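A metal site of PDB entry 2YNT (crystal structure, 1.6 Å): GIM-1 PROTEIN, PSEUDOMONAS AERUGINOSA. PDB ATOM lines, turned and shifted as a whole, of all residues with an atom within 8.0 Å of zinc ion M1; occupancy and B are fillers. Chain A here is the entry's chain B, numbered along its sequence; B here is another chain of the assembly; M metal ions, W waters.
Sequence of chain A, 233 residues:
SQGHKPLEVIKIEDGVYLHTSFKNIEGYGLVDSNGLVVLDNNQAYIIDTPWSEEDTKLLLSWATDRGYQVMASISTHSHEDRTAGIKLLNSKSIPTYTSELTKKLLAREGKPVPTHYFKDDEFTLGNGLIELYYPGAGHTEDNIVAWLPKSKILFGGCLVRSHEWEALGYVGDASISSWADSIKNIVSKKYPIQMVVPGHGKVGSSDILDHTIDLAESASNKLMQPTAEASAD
Zinc ion M1 is bound by water W1, a ring nitrogen (ND1) of His 79, a ring nitrogen (NE2) of His 139 and a ring nitrogen (NE2) of His 77.
N of His 139 lies within hydrogen-bond range of OD1 of Asn 143.
The side-chain carboxylate (OD2) of Asp 173 sits at hydrogen-bond distance from a ring nitrogen (NE2) of His 79, 2.7 Å away.
Within 4 Å of zinc ion M1: His 77, His 79 and His 139.
The nearest printed residue that does not touch zinc ion M1 is Asp 81 (4.03 Å).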
ATOM      1  N   THR A  76      10.232 -20.158  16.498  1.00  0.00           N
ATOM      2  CA  THR A  76      10.488 -19.017  17.398  1.00  0.00           C
ATOM      3  C   THR A  76      11.600 -19.233  18.433  1.00  0.00           C
ATOM      4  O   THR A  76      11.945 -18.316  19.180  1.00  0.00           O
ATOM      5  CB  THR A  76       9.191 -18.555  18.091  1.00  0.00           C
ATOM      6  OG1 THR A  76       8.644 -19.633  18.863  1.00  0.00           O
ATOM      7  CG2 THR A  76       8.173 -18.101  17.046  1.00  0.00           C
ATOM      8  N   HIS A  77      12.131 -20.454  18.478  1.00  0.00           N
ATOM      9  CA  HIS A  77      13.430 -20.747  19.096  1.00  0.00           C
ATOM     10  C   HIS A  77      13.790 -22.172  18.733  1.00  0.00           C
ATOM     11  O   HIS A  77      13.037 -22.823  18.016  1.00  0.00           O
ATOM     12  CB  HIS A  77      13.493 -20.483  20.634  1.00  0.00           C
ATOM     13  CG  HIS A  77      12.581 -21.333  21.475  1.00  0.00           C
ATOM     14  ND1 HIS A  77      11.245 -21.042  21.654  1.00  0.00           N
ATOM     15  CD2 HIS A  77      12.840 -22.407  22.259  1.00  0.00           C
ATOM     16  CE1 HIS A  77      10.704 -21.922  22.483  1.00  0.00           C
ATOM     17  NE2 HIS A  77      11.650 -22.764  22.862  1.00  0.00           N
ATOM     18  N   SER A  78      14.933 -22.668  19.215  1.00  0.00           N
ATOM     19  CA  SER A  78      15.491 -23.916  18.700  1.00  0.00           C
ATOM     20  C   SER A  78      14.960 -25.215  19.303  1.00  0.00           C
ATOM     21  O   SER A  78      15.233 -26.295  18.787  1.00  0.00           O
ATOM     22  CB  SER A  78      17.011 -23.911  18.822  1.00  0.00           C
ATOM     23  OG  SER A  78      17.404 -24.092  20.177  1.00  0.00           O
ATOM     24  N   HIS A  79      14.217 -25.116  20.413  1.00  0.00           N
ATOM     25  CA  HIS A  79      13.712 -26.312  21.080  1.00  0.00           C
ATOM     26  C   HIS A  79      12.857 -27.181  20.147  1.00  0.00           C
ATOM     27  O   HIS A  79      12.190 -26.660  19.227  1.00  0.00           O
ATOM     28  CB  HIS A  79      12.913 -25.928  22.323  1.00  0.00           C
ATOM     29  CG  HIS A  79      13.769 -25.524  23.484  1.00  0.00           C
ATOM     30  ND1 HIS A  79      13.261 -24.822  24.547  1.00  0.00           N
ATOM     31  CD2 HIS A  79      15.079 -25.744  23.745  1.00  0.00           C
ATOM     32  CE1 HIS A  79      14.236 -24.613  25.425  1.00  0.00           C
ATOM     33  NE2 HIS A  79      15.336 -25.173  24.971  1.00  0.00           N
ATOM     34  N   GLU A  80      12.875 -28.492  20.392  1.00  0.00           N
ATOM     35  CA  GLU A  80      12.155 -29.449  19.540  1.00  0.00           C
ATOM     36  C   GLU A  80      10.656 -29.143  19.405  1.00  0.00           C
ATOM     37  O   GLU A  80      10.068 -29.394  18.340  1.00  0.00           O
ATOM     38  CB  GLU A  80      12.357 -30.866  20.080  1.00  0.00           C
ATOM     39  CG  GLU A  80      11.793 -31.972  19.203  1.00  0.00           C
ATOM     40  OE1 GLU A  80      12.193 -33.423  21.052  1.00  0.00           O
ATOM     41  OE2 GLU A  80      11.878 -34.346  19.090  1.00  0.00           O
ATOM     42  N   ASP A  81      10.030 -28.602  20.448  1.00  0.00           N
ATOM     43  CA  ASP A  81       8.598 -28.302  20.344  1.00  0.00           C
ATOM     44  C   ASP A  81       8.294 -27.151  19.379  1.00  0.00           C
ATOM     45  O   ASP A  81       7.142 -26.953  19.033  1.00  0.00           O
ATOM     46  CB  ASP A  81       7.939 -28.088  21.720  1.00  0.00           C
ATOM     47  CG  ASP A  81       8.563 -26.975  22.517  1.00  0.00           C
ATOM     48  OD1 ASP A  81       9.702 -27.157  23.015  1.00  0.00           O
ATOM     49  OD2 ASP A  81       7.903 -25.915  22.693  1.00  0.00           O
ATOM     50  N   ARG A  82       9.317 -26.420  18.944  1.00  0.00           N
ATOM     51  CA  ARG A  82       9.130 -25.364  17.939  1.00  0.00           C
ATOM     52  C   ARG A  82       9.559 -25.794  16.538  1.00  0.00           C
ATOM     53  O   ARG A  82       9.181 -25.148  15.544  1.00  0.00           O
ATOM     54  CB  ARG A  82       9.960 -24.123  18.299  1.00  0.00           C
ATOM     55  CG  ARG A  82       9.795 -23.566  19.698  1.00  0.00           C
ATOM     56  CD  ARG A  82       8.433 -22.961  19.928  1.00  0.00           C
ATOM     57  NE  ARG A  82       7.521 -23.928  20.547  1.00  0.00           N
ATOM     58  CZ  ARG A  82       6.203 -23.795  20.603  1.00  0.00           C
ATOM     59  NH1 ARG A  82       5.611 -22.757  20.031  1.00  0.00           N
ATOM     60  NH2 ARG A  82       5.477 -24.715  21.228  1.00  0.00           N
ATOM     61  N   HIS A 139      12.935 -17.233  28.148  1.00  0.00           N
ATOM     62  CA  HIS A 139      12.800 -18.686  28.116  1.00  0.00           C
ATOM     63  C   HIS A 139      14.062 -19.320  27.504  1.00  0.00           C
ATOM     64  O   HIS A 139      14.586 -20.332  28.016  1.00  0.00           O
ATOM     65  CB  HIS A 139      11.567 -19.039  27.290  1.00  0.00           C
ATOM     66  CG  HIS A 139      11.460 -20.485  26.949  1.00  0.00           C
ATOM     67  ND1 HIS A 139      11.094 -21.442  27.873  1.00  0.00           N
ATOM     68  CD2 HIS A 139      11.693 -21.146  25.796  1.00  0.00           C
ATOM     69  CE1 HIS A 139      11.093 -22.635  27.284  1.00  0.00           C
ATOM     70  NE2 HIS A 139      11.450 -22.473  26.027  1.00  0.00           N
ATOM     71  N   THR A 140      14.538 -18.743  26.409  1.00  0.00           N
ATOM     72  CA  THR A 140      15.850 -19.071  25.851  1.00  0.00           C
ATOM     73  C   THR A 140      16.563 -17.796  25.406  1.00  0.00           C
ATOM     74  O   THR A 140      15.986 -16.697  25.447  1.00  0.00           O
ATOM     75  CB  THR A 140      15.740 -19.988  24.626  1.00  0.00           C
ATOM     76  OG1 THR A 140      14.864 -19.386  23.668  1.00  0.00           O
ATOM     77  CG2 THR A 140      15.219 -21.366  25.033  1.00  0.00           C
ATOM     78  N   ASP A 142      17.359 -17.114  22.431  1.00  0.00           N
ATOM     79  CA  ASP A 142      17.007 -16.791  21.042  1.00  0.00           C
ATOM     80  C   ASP A 142      15.533 -16.561  20.809  1.00  0.00           C
ATOM     81  O   ASP A 142      15.127 -16.277  19.680  1.00  0.00           O
ATOM     82  CB  ASP A 142      17.492 -17.917  20.100  1.00  0.00           C
ATOM     83  CG  ASP A 142      16.890 -19.289  20.438  1.00  0.00           C
ATOM     84  OD1 ASP A 142      16.726 -19.601  21.636  1.00  0.00           O
ATOM     85  OD2 ASP A 142      16.583 -20.064  19.508  1.00  0.00           O
ATOM     86  N   ASN A 143      14.715 -16.672  21.852  1.00  0.00           N
ATOM     87  CA  ASN A 143      13.263 -16.569  21.652  1.00  0.00           C
ATOM     88  C   ASN A 143      12.781 -15.282  20.969  1.00  0.00           C
ATOM     89  O   ASN A 143      13.208 -14.178  21.316  1.00  0.00           O
ATOM     90  CB  ASN A 143      12.458 -16.870  22.945  1.00  0.00           C
ATOM     91  CG  ASN A 143      12.907 -16.058  24.174  1.00  0.00           C
ATOM     92  OD1 ASN A 143      12.762 -16.538  25.307  1.00  0.00           O
ATOM     93  ND2 ASN A 143      13.383 -14.824  23.966  1.00  0.00           N
ATOM     94  N   GLY A 157       4.776 -17.320  22.147  1.00  0.00           N
ATOM     95  CA  GLY A 157       5.579 -18.538  22.198  1.00  0.00           C
ATOM     96  C   GLY A 157       5.926 -18.870  23.634  1.00  0.00           C
ATOM     97  O   GLY A 157       5.188 -18.532  24.575  1.00  0.00           O
ATOM     98  N   CYS A 158       7.063 -19.513  23.822  1.00  0.00           N
ATOM     99  CA  CYS A 158       7.375 -20.108  25.124  1.00  0.00           C
ATOM    100  C   CYS A 158       7.982 -19.095  26.076  1.00  0.00           C
ATOM    101  O   CYS A 158       8.220 -19.386  27.254  1.00  0.00           O
ATOM    102  CB  CYS A 158       8.283 -21.329  24.913  1.00  0.00           C
ATOM    103  SG  CYS A 158       7.543 -22.490  23.717  1.00  0.00           S
ATOM    104  N   LEU A 159       8.206 -17.884  25.576  1.00  0.00           N
ATOM    105  CA  LEU A 159       8.649 -16.765  26.386  1.00  0.00           C
ATOM    106  C   LEU A 159       7.546 -16.262  27.313  1.00  0.00           C
ATOM    107  O   LEU A 159       7.829 -15.640  28.334  1.00  0.00           O
ATOM    108  CB  LEU A 159       9.111 -15.618  25.477  1.00  0.00           C
ATOM    109  CG  LEU A 159       9.532 -14.283  26.095  1.00  0.00           C
ATOM    110  CD1 LEU A 159      10.749 -14.449  27.007  1.00  0.00           C
ATOM    111  CD2 LEU A 159       9.829 -13.299  24.982  1.00  0.00           C
ATOM    112  N   TYR A 170      10.061 -24.957  31.847  1.00  0.00           N
ATOM    113  CA  TYR A 170      11.412 -25.479  31.640  1.00  0.00           C
ATOM    114  C   TYR A 170      12.433 -24.348  31.528  1.00  0.00           C
ATOM    115  O   TYR A 170      12.341 -23.513  30.625  1.00  0.00           O
ATOM    116  CB  TYR A 170      11.484 -26.366  30.397  1.00  0.00           C
ATOM    117  CG  TYR A 170      12.886 -26.880  30.138  1.00  0.00           C
ATOM    118  CD1 TYR A 170      13.408 -27.924  30.902  1.00  0.00           C
ATOM    119  CD2 TYR A 170      13.694 -26.324  29.138  1.00  0.00           C
ATOM    120  CE1 TYR A 170      14.691 -28.394  30.686  1.00  0.00           C
ATOM    121  CE2 TYR A 170      14.978 -26.798  28.908  1.00  0.00           C
ATOM    122  CZ  TYR A 170      15.470 -27.825  29.694  1.00  0.00           C
ATOM    123  OH  TYR A 170      16.735 -28.308  29.473  1.00  0.00           O
ATOM    124  N   ASP A 173      17.502 -23.785  29.660  1.00  0.00           N
ATOM    125  CA  ASP A 173      18.204 -22.899  28.714  1.00  0.00           C
ATOM    126  C   ASP A 173      17.820 -21.436  28.910  1.00  0.00           C
ATOM    127  O   ASP A 173      18.068 -20.594  28.033  1.00  0.00           O
ATOM    128  CB  ASP A 173      17.919 -23.322  27.275  1.00  0.00           C
ATOM    129  CG  ASP A 173      18.413 -24.723  26.967  1.00  0.00           C
ATOM    130  OD1 ASP A 173      19.572 -25.040  27.333  1.00  0.00           O
ATOM    131  OD2 ASP A 173      17.652 -25.505  26.371  1.00  0.00           O
ATOM    132  N   HIS A 200       2.858 -22.983  25.456  1.00  0.00           N
ATOM    133  CA  HIS A 200       2.293 -24.084  26.234  1.00  0.00           C
ATOM    134  C   HIS A 200       1.162 -23.553  27.089  1.00  0.00           C
ATOM    135  O   HIS A 200       1.304 -22.519  27.754  1.00  0.00           O
ATOM    136  CB  HIS A 200       3.379 -24.723  27.110  1.00  0.00           C
ATOM    137  CG  HIS A 200       4.585 -25.156  26.347  1.00  0.00           C
ATOM    138  ND1 HIS A 200       4.627 -26.322  25.608  1.00  0.00           N
ATOM    139  CD2 HIS A 200       5.804 -24.572  26.191  1.00  0.00           C
ATOM    140  CE1 HIS A 200       5.808 -26.429  25.028  1.00  0.00           C
ATOM    141  NE2 HIS A 200       6.548 -25.385  25.369  1.00  0.00           N
ATOM    142  N   GLU B  26      11.793 -30.889  28.971  1.00  0.00           N
ATOM    143  CA  GLU B  26      11.591 -29.806  28.016  1.00  0.00           C
ATOM    144  C   GLU B  26      10.122 -29.825  27.579  1.00  0.00           C
ATOM    145  O   GLU B  26       9.523 -30.895  27.409  1.00  0.00           O
ATOM    146  CB  GLU B  26      12.515 -29.980  26.798  1.00  0.00           C
ATOM    147  CG  GLU B  26      13.147 -28.694  26.297  1.00  0.00           C
ATOM    148  CD  GLU B  26      14.078 -28.932  25.110  1.00  0.00           C
ATOM    149  OE1 GLU B  26      13.567 -29.130  23.986  1.00  0.00           O
ATOM    150  OE2 GLU B  26      15.312 -28.932  25.316  1.00  0.00           O
ATOM    151  N   GLY B  27       9.536 -28.656  27.427  1.00  0.00           N
ATOM    152  CA  GLY B  27       8.130 -28.579  27.089  1.00  0.00           C
ATOM    153  C   GLY B  27       7.285 -28.396  28.333  1.00  0.00           C
ATOM    154  O   GLY B  27       6.165 -27.899  28.237  1.00  0.00           O
ATOM    155  N   TYR B  28       7.807 -28.780  29.493  1.00  0.00           N
ATOM    156  CA  TYR B  28       7.063 -28.608  30.758  1.00  0.00           C
ATOM    157  C   TYR B  28       7.884 -28.017  31.916  1.00  0.00           C
ATOM    158  O   TYR B  28       7.460 -27.034  32.538  1.00  0.00           O
ATOM    159  CB  TYR B  28       6.412 -29.916  31.219  1.00  0.00           C
ATOM    160  CG  TYR B  28       5.732 -29.737  32.553  1.00  0.00           C
ATOM    161  CD1 TYR B  28       4.517 -29.080  32.648  1.00  0.00           C
ATOM    162  CD2 TYR B  28       6.332 -30.181  33.727  1.00  0.00           C
ATOM    163  CE1 TYR B  28       3.907 -28.873  33.865  1.00  0.00           C
ATOM    164  CE2 TYR B  28       5.726 -29.989  34.950  1.00  0.00           C
ATOM    165  CZ  TYR B  28       4.515 -29.333  35.007  1.00  0.00           C
ATOM    166  OH  TYR B  28       3.905 -29.140  36.221  1.00  0.00           O
HETATM  167 ZN    ZN M   1      11.487 -23.887  24.563  1.00  0.00          ZN
HETATM  168 ZN    ZN M   2       8.073 -24.615  24.260  1.00  0.00          ZN
HETATM  169  O   HOH W   1       9.999 -25.045  24.767  1.00  0.00           O
